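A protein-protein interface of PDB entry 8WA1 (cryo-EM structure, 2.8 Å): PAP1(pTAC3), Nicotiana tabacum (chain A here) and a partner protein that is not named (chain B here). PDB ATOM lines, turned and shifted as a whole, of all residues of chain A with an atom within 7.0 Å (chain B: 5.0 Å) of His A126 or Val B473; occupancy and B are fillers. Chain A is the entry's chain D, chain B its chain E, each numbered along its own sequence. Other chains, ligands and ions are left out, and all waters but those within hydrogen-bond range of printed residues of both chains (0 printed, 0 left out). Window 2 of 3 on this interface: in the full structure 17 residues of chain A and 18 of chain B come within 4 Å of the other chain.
CG2 of Val B473 touches NE2 of His A126 (3.7 Å). CG1 of Val B473 touches O of Arg A129 (3.97 Å). CG2 of Thr B477 touches NE of Arg A129 (3.4 Å). Arg A130 touches Glu B469. Val B473 touches Arg A130 (CG1 to CA, 3.7 Å). Ser A133 touches Val B473. Asn B476 touches Ser A133 (OD1 to OG, 3.5 Å).
The side-chain hydroxyl of Thr B477 lies within hydrogen-bond range of the backbone carbonyl oxygen of Ala B474. OE1 of Glu A134 is in salt-bridge range of NH1 of Arg A130 (3.7 Å). O of Val B472 lies close to OD1 of Asn B476 (2.9 Å). OG of Ser A133 sits at hydrogen-bond distance from O of Arg A129 (2.9 Å). The backbone carbonyl oxygen (O) of Val B473 sits at hydrogen-bond distance from the side-chain hydroxyl (OG1) of Thr B477 (3.1 Å).
Of the 17 printed residues of chain A, 5 touch a printed residue of chain B. Hydrophobic or aromatic side chains of chain A within 4 Å of the printed part of chain B: His A126. Of the 10 printed residues of chain B, 4 touch a printed residue of chain A. Hydrophobic or aromatic side chains of chain B that line the printed part of chain A: Val B473. Among the printed residues, 8 pairs touch across the chains. Among the printed residues, no Asp or Glu carboxylate lies within 4 Å of a Lys or Arg side-chain nitrogen of the other chain.
His A126 touches just one residue of chain B: Val B473. Printed residues of chain B within 4 Å of Arg A129: Val B473 and Thr B477. Of the printed residues of chain B, Arg A130 touches Glu B469 and Val B473. Printed residues of chain B within 4 Å of Ser A133: Val B473 (3.5 Å) and Asn B476 (3.5 Å). Printed residues of chain B within 4 Å of Glu A134: Glu B469 (2.9 Å). Val B473 touches four residues of chain A. Of the printed residues of chain A, Thr B477 touches Arg A129 (3.4 Å). The nearest residue of chain A that does not touch Val B473 is Glu A131 (6.0 Å).
The side-chain carboxylate (OE1) of Glu B469 lies close to the side-chain carboxylate (OE1) of Glu A134, at 2.9 Å.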
ATOM      1  N   PHE A 108     -23.965   6.038 -14.930  1.00  0.00           N
ATOM      2  CA  PHE A 108     -23.361   5.175 -13.924  1.00  0.00           C
ATOM      3  C   PHE A 108     -24.397   4.564 -12.991  1.00  0.00           C
ATOM      4  O   PHE A 108     -24.112   3.544 -12.356  1.00  0.00           O
ATOM      5  CB  PHE A 108     -22.325   5.954 -13.111  1.00  0.00           C
ATOM      6  CG  PHE A 108     -21.145   6.412 -13.918  1.00  0.00           C
ATOM      7  CD1 PHE A 108     -20.030   5.603 -14.057  1.00  0.00           C
ATOM      8  CD2 PHE A 108     -21.152   7.649 -14.539  1.00  0.00           C
ATOM      9  CE1 PHE A 108     -18.943   6.020 -14.800  1.00  0.00           C
ATOM     10  CE2 PHE A 108     -20.068   8.072 -15.284  1.00  0.00           C
ATOM     11  CZ  PHE A 108     -18.962   7.256 -15.415  1.00  0.00           C
ATOM     12  N   PHE A 111     -25.028   1.152 -14.389  1.00  0.00           N
ATOM     13  CA  PHE A 111     -23.938   0.239 -14.060  1.00  0.00           C
ATOM     14  C   PHE A 111     -24.019  -0.205 -12.603  1.00  0.00           C
ATOM     15  O   PHE A 111     -23.848  -1.391 -12.288  1.00  0.00           O
ATOM     16  CB  PHE A 111     -22.597   0.917 -14.346  1.00  0.00           C
ATOM     17  CG  PHE A 111     -21.523  -0.027 -14.805  1.00  0.00           C
ATOM     18  CD1 PHE A 111     -21.792  -1.374 -14.976  1.00  0.00           C
ATOM     19  CD2 PHE A 111     -20.243   0.434 -15.063  1.00  0.00           C
ATOM     20  CE1 PHE A 111     -20.805  -2.245 -15.399  1.00  0.00           C
ATOM     21  CE2 PHE A 111     -19.251  -0.430 -15.484  1.00  0.00           C
ATOM     22  CZ  PHE A 111     -19.533  -1.773 -15.653  1.00  0.00           C
ATOM     23  N   HIS A 115     -24.693  -4.008 -11.246  1.00  0.00           N
ATOM     24  CA  HIS A 115     -23.816  -4.711 -10.316  1.00  0.00           C
ATOM     25  C   HIS A 115     -24.566  -5.139  -9.060  1.00  0.00           C
ATOM     26  O   HIS A 115     -24.252  -6.176  -8.463  1.00  0.00           O
ATOM     27  CB  HIS A 115     -22.623  -3.828  -9.956  1.00  0.00           C
ATOM     28  CG  HIS A 115     -21.544  -3.816 -10.996  1.00  0.00           C
ATOM     29  ND1 HIS A 115     -20.826  -2.683 -11.310  1.00  0.00           N
ATOM     30  CD2 HIS A 115     -21.055  -4.802 -11.785  1.00  0.00           C
ATOM     31  CE1 HIS A 115     -19.943  -2.970 -12.250  1.00  0.00           C
ATOM     32  NE2 HIS A 115     -20.063  -4.249 -12.556  1.00  0.00           N
ATOM     33  N   ASN A 121     -20.555  -6.591  -5.131  1.00  0.00           N
ATOM     34  CA  ASN A 121     -20.251  -5.362  -4.408  1.00  0.00           C
ATOM     35  C   ASN A 121     -18.989  -4.672  -4.911  1.00  0.00           C
ATOM     36  O   ASN A 121     -18.945  -3.441  -4.984  1.00  0.00           O
ATOM     37  CB  ASN A 121     -20.128  -5.654  -2.907  1.00  0.00           C
ATOM     38  CG  ASN A 121     -19.136  -6.759  -2.607  1.00  0.00           C
ATOM     39  OD1 ASN A 121     -19.473  -7.942  -2.663  1.00  0.00           O
ATOM     40  ND2 ASN A 121     -17.905  -6.379  -2.284  1.00  0.00           N
ATOM     41  N   ASP A 122     -17.951  -5.442  -5.247  1.00  0.00           N
ATOM     42  CA  ASP A 122     -16.702  -4.839  -5.704  1.00  0.00           C
ATOM     43  C   ASP A 122     -16.882  -4.133  -7.043  1.00  0.00           C
ATOM     44  O   ASP A 122     -16.312  -3.059  -7.266  1.00  0.00           O
ATOM     45  CB  ASP A 122     -15.611  -5.907  -5.794  1.00  0.00           C
ATOM     46  CG  ASP A 122     -15.267  -6.501  -4.443  1.00  0.00           C
ATOM     47  OD1 ASP A 122     -15.379  -5.778  -3.430  1.00  0.00           O
ATOM     48  OD2 ASP A 122     -14.888  -7.690  -4.391  1.00  0.00           O
ATOM     49  N   GLY A 123     -17.680  -4.713  -7.943  1.00  0.00           N
ATOM     50  CA  GLY A 123     -17.965  -4.038  -9.199  1.00  0.00           C
ATOM     51  C   GLY A 123     -18.732  -2.746  -9.000  1.00  0.00           C
ATOM     52  O   GLY A 123     -18.470  -1.746  -9.672  1.00  0.00           O
ATOM     53  N   ALA A 124     -19.687  -2.747  -8.068  1.00  0.00           N
ATOM     54  CA  ALA A 124     -20.440  -1.531  -7.782  1.00  0.00           C
ATOM     55  C   ALA A 124     -19.547  -0.464  -7.162  1.00  0.00           C
ATOM     56  O   ALA A 124     -19.682   0.724  -7.477  1.00  0.00           O
ATOM     57  CB  ALA A 124     -21.621  -1.848  -6.867  1.00  0.00           C
ATOM     58  N   MET A 125     -18.626  -0.866  -6.284  1.00  0.00           N
ATOM     59  CA  MET A 125     -17.661   0.080  -5.734  1.00  0.00           C
ATOM     60  C   MET A 125     -16.735   0.640  -6.806  1.00  0.00           C
ATOM     61  O   MET A 125     -16.430   1.837  -6.779  1.00  0.00           O
ATOM     62  CB  MET A 125     -16.836  -0.585  -4.632  1.00  0.00           C
ATOM     63  CG  MET A 125     -17.627  -0.941  -3.382  1.00  0.00           C
ATOM     64  SD  MET A 125     -18.169   0.510  -2.455  1.00  0.00           S
ATOM     65  CE  MET A 125     -16.591   1.211  -1.978  1.00  0.00           C
ATOM     66  N   HIS A 126     -16.294  -0.195  -7.752  1.00  0.00           N
ATOM     67  CA  HIS A 126     -15.472   0.302  -8.851  1.00  0.00           C
ATOM     68  C   HIS A 126     -16.254   1.277  -9.723  1.00  0.00           C
ATOM     69  O   HIS A 126     -15.715   2.301 -10.156  1.00  0.00           O
ATOM     70  CB  HIS A 126     -14.950  -0.867  -9.688  1.00  0.00           C
ATOM     71  CG  HIS A 126     -14.245  -0.449 -10.942  1.00  0.00           C
ATOM     72  ND1 HIS A 126     -14.866  -0.423 -12.173  1.00  0.00           N
ATOM     73  CD2 HIS A 126     -12.971  -0.045 -11.156  1.00  0.00           C
ATOM     74  CE1 HIS A 126     -14.006  -0.019 -13.090  1.00  0.00           C
ATOM     75  NE2 HIS A 126     -12.848   0.216 -12.500  1.00  0.00           N
ATOM     76  N   ALA A 127     -17.530   0.980  -9.980  1.00  0.00           N
ATOM     77  CA  ALA A 127     -18.357   1.889 -10.767  1.00  0.00           C
ATOM     78  C   ALA A 127     -18.557   3.215 -10.044  1.00  0.00           C
ATOM     79  O   ALA A 127     -18.515   4.284 -10.667  1.00  0.00           O
ATOM     80  CB  ALA A 127     -19.705   1.237 -11.074  1.00  0.00           C
ATOM     81  N   LEU A 128     -18.774   3.166  -8.729  1.00  0.00           N
ATOM     82  CA  LEU A 128     -18.913   4.395  -7.954  1.00  0.00           C
ATOM     83  C   LEU A 128     -17.625   5.208  -7.977  1.00  0.00           C
ATOM     84  O   LEU A 128     -17.662   6.437  -8.109  1.00  0.00           O
ATOM     85  CB  LEU A 128     -19.314   4.070  -6.517  1.00  0.00           C
ATOM     86  CG  LEU A 128     -19.490   5.287  -5.606  1.00  0.00           C
ATOM     87  CD1 LEU A 128     -20.766   6.041  -5.954  1.00  0.00           C
ATOM     88  CD2 LEU A 128     -19.473   4.886  -4.140  1.00  0.00           C
ATOM     89  N   ARG A 129     -16.476   4.540  -7.844  1.00  0.00           N
ATOM     90  CA  ARG A 129     -15.204   5.251  -7.900  1.00  0.00           C
ATOM     91  C   ARG A 129     -14.961   5.862  -9.273  1.00  0.00           C
ATOM     92  O   ARG A 129     -14.427   6.971  -9.370  1.00  0.00           O
ATOM     93  CB  ARG A 129     -14.057   4.315  -7.518  1.00  0.00           C
ATOM     94  CG  ARG A 129     -13.936   4.086  -6.021  1.00  0.00           C
ATOM     95  CD  ARG A 129     -12.672   3.323  -5.670  1.00  0.00           C
ATOM     96  NE  ARG A 129     -12.807   1.887  -5.902  1.00  0.00           N
ATOM     97  CZ  ARG A 129     -13.233   1.024  -4.988  1.00  0.00           C
ATOM     98  NH1 ARG A 129     -13.570   1.452  -3.779  1.00  0.00           N
ATOM     99  NH2 ARG A 129     -13.325  -0.266  -5.278  1.00  0.00           N
ATOM    100  N   ARG A 130     -15.353   5.166 -10.341  1.00  0.00           N
ATOM    101  CA  ARG A 130     -15.229   5.736 -11.679  1.00  0.00           C
ATOM    102  C   ARG A 130     -16.122   6.961 -11.836  1.00  0.00           C
ATOM    103  O   ARG A 130     -15.700   7.985 -12.387  1.00  0.00           O
ATOM    104  CB  ARG A 130     -15.565   4.682 -12.735  1.00  0.00           C
ATOM    105  CG  ARG A 130     -14.550   3.554 -12.838  1.00  0.00           C
ATOM    106  CD  ARG A 130     -13.905   3.494 -14.217  1.00  0.00           C
ATOM    107  NE  ARG A 130     -14.861   3.154 -15.268  1.00  0.00           N
ATOM    108  CZ  ARG A 130     -15.425   4.040 -16.084  1.00  0.00           C
ATOM    109  NH1 ARG A 130     -15.130   5.328 -15.974  1.00  0.00           N
ATOM    110  NH2 ARG A 130     -16.283   3.639 -17.012  1.00  0.00           N
ATOM    111  N   GLU A 131     -17.365   6.873 -11.354  1.00  0.00           N
ATOM    112  CA  GLU A 131     -18.272   8.014 -11.434  1.00  0.00           C
ATOM    113  C   GLU A 131     -17.743   9.200 -10.635  1.00  0.00           C
ATOM    114  O   GLU A 131     -17.870  10.354 -11.062  1.00  0.00           O
ATOM    115  CB  GLU A 131     -19.664   7.614 -10.945  1.00  0.00           C
ATOM    116  CG  GLU A 131     -20.699   8.724 -11.049  1.00  0.00           C
ATOM    117  CD  GLU A 131     -22.055   8.314 -10.504  1.00  0.00           C
ATOM    118  OE1 GLU A 131     -22.171   7.186  -9.983  1.00  0.00           O
ATOM    119  OE2 GLU A 131     -23.004   9.120 -10.598  1.00  0.00           O
ATOM    120  N   LEU A 132     -17.151   8.935  -9.469  1.00  0.00           N
ATOM    121  CA  LEU A 132     -16.615  10.014  -8.645  1.00  0.00           C
ATOM    122  C   LEU A 132     -15.374  10.631  -9.281  1.00  0.00           C
ATOM    123  O   LEU A 132     -15.179  11.851  -9.226  1.00  0.00           O
ATOM    124  CB  LEU A 132     -16.303   9.494  -7.242  1.00  0.00           C
ATOM    125  CG  LEU A 132     -15.924  10.535  -6.188  1.00  0.00           C
ATOM    126  CD1 LEU A 132     -17.007  11.595  -6.077  1.00  0.00           C
ATOM    127  CD2 LEU A 132     -15.680   9.873  -4.841  1.00  0.00           C
ATOM    128  N   SER A 133     -14.519   9.801  -9.887  1.00  0.00           N
ATOM    129  CA  SER A 133     -13.357  10.323 -10.598  1.00  0.00           C
ATOM    130  C   SER A 133     -13.781  11.124 -11.821  1.00  0.00           C
ATOM    131  O   SER A 133     -13.056  12.021 -12.268  1.00  0.00           O
ATOM    132  CB  SER A 133     -12.430   9.176 -11.004  1.00  0.00           C
ATOM    133  OG  SER A 133     -11.969   8.466  -9.867  1.00  0.00           O
ATOM    134  N   GLU A 134     -14.949  10.809 -12.381  1.00  0.00           N
ATOM    135  CA  GLU A 134     -15.478  11.569 -13.505  1.00  0.00           C
ATOM    136  C   GLU A 134     -15.836  13.004 -13.138  1.00  0.00           C
ATOM    137  O   GLU A 134     -16.069  13.813 -14.043  1.00  0.00           O
ATOM    138  CB  GLU A 134     -16.708  10.861 -14.078  1.00  0.00           C
ATOM    139  CG  GLU A 134     -16.693  10.702 -15.590  1.00  0.00           C
ATOM    140  CD  GLU A 134     -15.673   9.684 -16.066  1.00  0.00           C
ATOM    141  OE1 GLU A 134     -15.132   8.936 -15.223  1.00  0.00           O
ATOM    142  OE2 GLU A 134     -15.413   9.631 -17.286  1.00  0.00           O
ATOM    143  N   GLU B 469      -9.664   5.971 -17.890  1.00  0.00           N
ATOM    144  CA  GLU B 469     -10.430   6.082 -16.652  1.00  0.00           C
ATOM    145  C   GLU B 469     -10.124   4.928 -15.705  1.00  0.00           C
ATOM    146  O   GLU B 469     -10.035   5.121 -14.486  1.00  0.00           O
ATOM    147  CB  GLU B 469     -11.925   6.140 -16.962  1.00  0.00           C
ATOM    148  CG  GLU B 469     -12.363   7.399 -17.694  1.00  0.00           C
ATOM    149  CD  GLU B 469     -12.340   8.632 -16.807  1.00  0.00           C
ATOM    150  OE1 GLU B 469     -12.335   8.478 -15.568  1.00  0.00           O
ATOM    151  OE2 GLU B 469     -12.326   9.756 -17.354  1.00  0.00           O
ATOM    152  N   GLU B 470      -9.959   3.720 -16.247  1.00  0.00           N
ATOM    153  CA  GLU B 470      -9.644   2.573 -15.403  1.00  0.00           C
ATOM    154  C   GLU B 470      -8.267   2.709 -14.768  1.00  0.00           C
ATOM    155  O   GLU B 470      -8.097   2.399 -13.585  1.00  0.00           O
ATOM    156  CB  GLU B 470      -9.745   1.282 -16.214  1.00  0.00           C
ATOM    157  CG  GLU B 470     -11.113   1.075 -16.850  1.00  0.00           C
ATOM    158  CD  GLU B 470     -11.288  -0.311 -17.437  1.00  0.00           C
ATOM    159  OE1 GLU B 470     -10.467  -1.199 -17.127  1.00  0.00           O
ATOM    160  OE2 GLU B 470     -12.249  -0.513 -18.209  1.00  0.00           O
ATOM    161  N   ALA B 471      -7.278   3.193 -15.523  1.00  0.00           N
ATOM    162  CA  ALA B 471      -5.960   3.424 -14.940  1.00  0.00           C
ATOM    163  C   ALA B 471      -6.012   4.516 -13.877  1.00  0.00           C
ATOM    164  O   ALA B 471      -5.343   4.418 -12.840  1.00  0.00           O
ATOM    165  CB  ALA B 471      -4.956   3.784 -16.035  1.00  0.00           C
ATOM    166  N   VAL B 472      -6.812   5.559 -14.111  1.00  0.00           N
ATOM    167  CA  VAL B 472      -6.919   6.644 -13.138  1.00  0.00           C
ATOM    168  C   VAL B 472      -7.546   6.146 -11.843  1.00  0.00           C
ATOM    169  O   VAL B 472      -7.063   6.452 -10.745  1.00  0.00           O
ATOM    170  CB  VAL B 472      -7.709   7.824 -13.736  1.00  0.00           C
ATOM    171  CG1 VAL B 472      -8.073   8.824 -12.648  1.00  0.00           C
ATOM    172  CG2 VAL B 472      -6.896   8.506 -14.824  1.00  0.00           C
ATOM    173  N   VAL B 473      -8.626   5.366 -11.942  1.00  0.00           N
ATOM    174  CA  VAL B 473      -9.275   4.874 -10.727  1.00  0.00           C
ATOM    175  C   VAL B 473      -8.406   3.823 -10.046  1.00  0.00           C
ATOM    176  O   VAL B 473      -8.429   3.682  -8.819  1.00  0.00           O
ATOM    177  CB  VAL B 473     -10.691   4.345 -11.030  1.00  0.00           C
ATOM    178  CG1 VAL B 473     -11.549   5.444 -11.642  1.00  0.00           C
ATOM    179  CG2 VAL B 473     -10.644   3.127 -11.935  1.00  0.00           C
ATOM    180  N   ALA B 474      -7.594   3.095 -10.820  1.00  0.00           N
ATOM    181  CA  ALA B 474      -6.647   2.164 -10.216  1.00  0.00           C
ATOM    182  C   ALA B 474      -5.584   2.908  -9.417  1.00  0.00           C
ATOM    183  O   ALA B 474      -5.230   2.500  -8.305  1.00  0.00           O
ATOM    184  CB  ALA B 474      -6.004   1.294 -11.293  1.00  0.00           C
ATOM    185  N   PHE B 475      -5.066   4.008  -9.968  1.00  0.00           N
ATOM    186  CA  PHE B 475      -4.112   4.827  -9.225  1.00  0.00           C
ATOM    187  C   PHE B 475      -4.757   5.431  -7.981  1.00  0.00           C
ATOM    188  O   PHE B 475      -4.132   5.493  -6.915  1.00  0.00           O
ATOM    189  CB  PHE B 475      -3.548   5.925 -10.128  1.00  0.00           C
ATOM    190  CG  PHE B 475      -2.620   6.872  -9.422  1.00  0.00           C
ATOM    191  CD1 PHE B 475      -1.322   6.497  -9.119  1.00  0.00           C
ATOM    192  CD2 PHE B 475      -3.044   8.144  -9.066  1.00  0.00           C
ATOM    193  CE1 PHE B 475      -0.466   7.368  -8.470  1.00  0.00           C
ATOM    194  CE2 PHE B 475      -2.193   9.019  -8.418  1.00  0.00           C
ATOM    195  CZ  PHE B 475      -0.903   8.629  -8.120  1.00  0.00           C
ATOM    196  N   ASN B 476      -6.010   5.878  -8.097  1.00  0.00           N
ATOM    197  CA  ASN B 476      -6.704   6.427  -6.937  1.00  0.00           C
ATOM    198  C   ASN B 476      -6.910   5.375  -5.853  1.00  0.00           C
ATOM    199  O   ASN B 476      -6.800   5.687  -4.663  1.00  0.00           O
ATOM    200  CB  ASN B 476      -8.046   7.029  -7.358  1.00  0.00           C
ATOM    201  CG  ASN B 476      -7.884   8.283  -8.197  1.00  0.00           C
ATOM    202  OD1 ASN B 476      -8.523   8.434  -9.238  1.00  0.00           O
ATOM    203  ND2 ASN B 476      -7.026   9.189  -7.745  1.00  0.00           N
ATOM    204  N   THR B 477      -7.204   4.132  -6.241  1.00  0.00           N
ATOM    205  CA  THR B 477      -7.317   3.061  -5.255  1.00  0.00           C
ATOM    206  C   THR B 477      -5.963   2.738  -4.639  1.00  0.00           C
ATOM    207  O   THR B 477      -5.875   2.432  -3.444  1.00  0.00           O
ATOM    208  CB  THR B 477      -7.922   1.811  -5.891  1.00  0.00           C
ATOM    209  OG1 THR B 477      -7.206   1.487  -7.089  1.00  0.00           O
ATOM    210  CG2 THR B 477      -9.386   2.032  -6.223  1.00  0.00           C
ATOM    211  N   MET B 478      -4.896   2.795  -5.440  1.00  0.00           N
ATOM    212  CA  MET B 478      -3.560   2.570  -4.898  1.00  0.00           C
ATOM    213  C   MET B 478      -3.192   3.653  -3.891  1.00  0.00           C
ATOM    214  O   MET B 478      -2.454   3.397  -2.932  1.00  0.00           O
ATOM    215  CB  MET B 478      -2.532   2.504  -6.031  1.00  0.00           C
ATOM    216  CG  MET B 478      -1.621   3.720  -6.149  1.00  0.00           C
ATOM    217  SD  MET B 478      -0.235   3.463  -7.272  1.00  0.00           S
ATOM    218  CE  MET B 478       0.664   2.180  -6.405  1.00  0.00           C
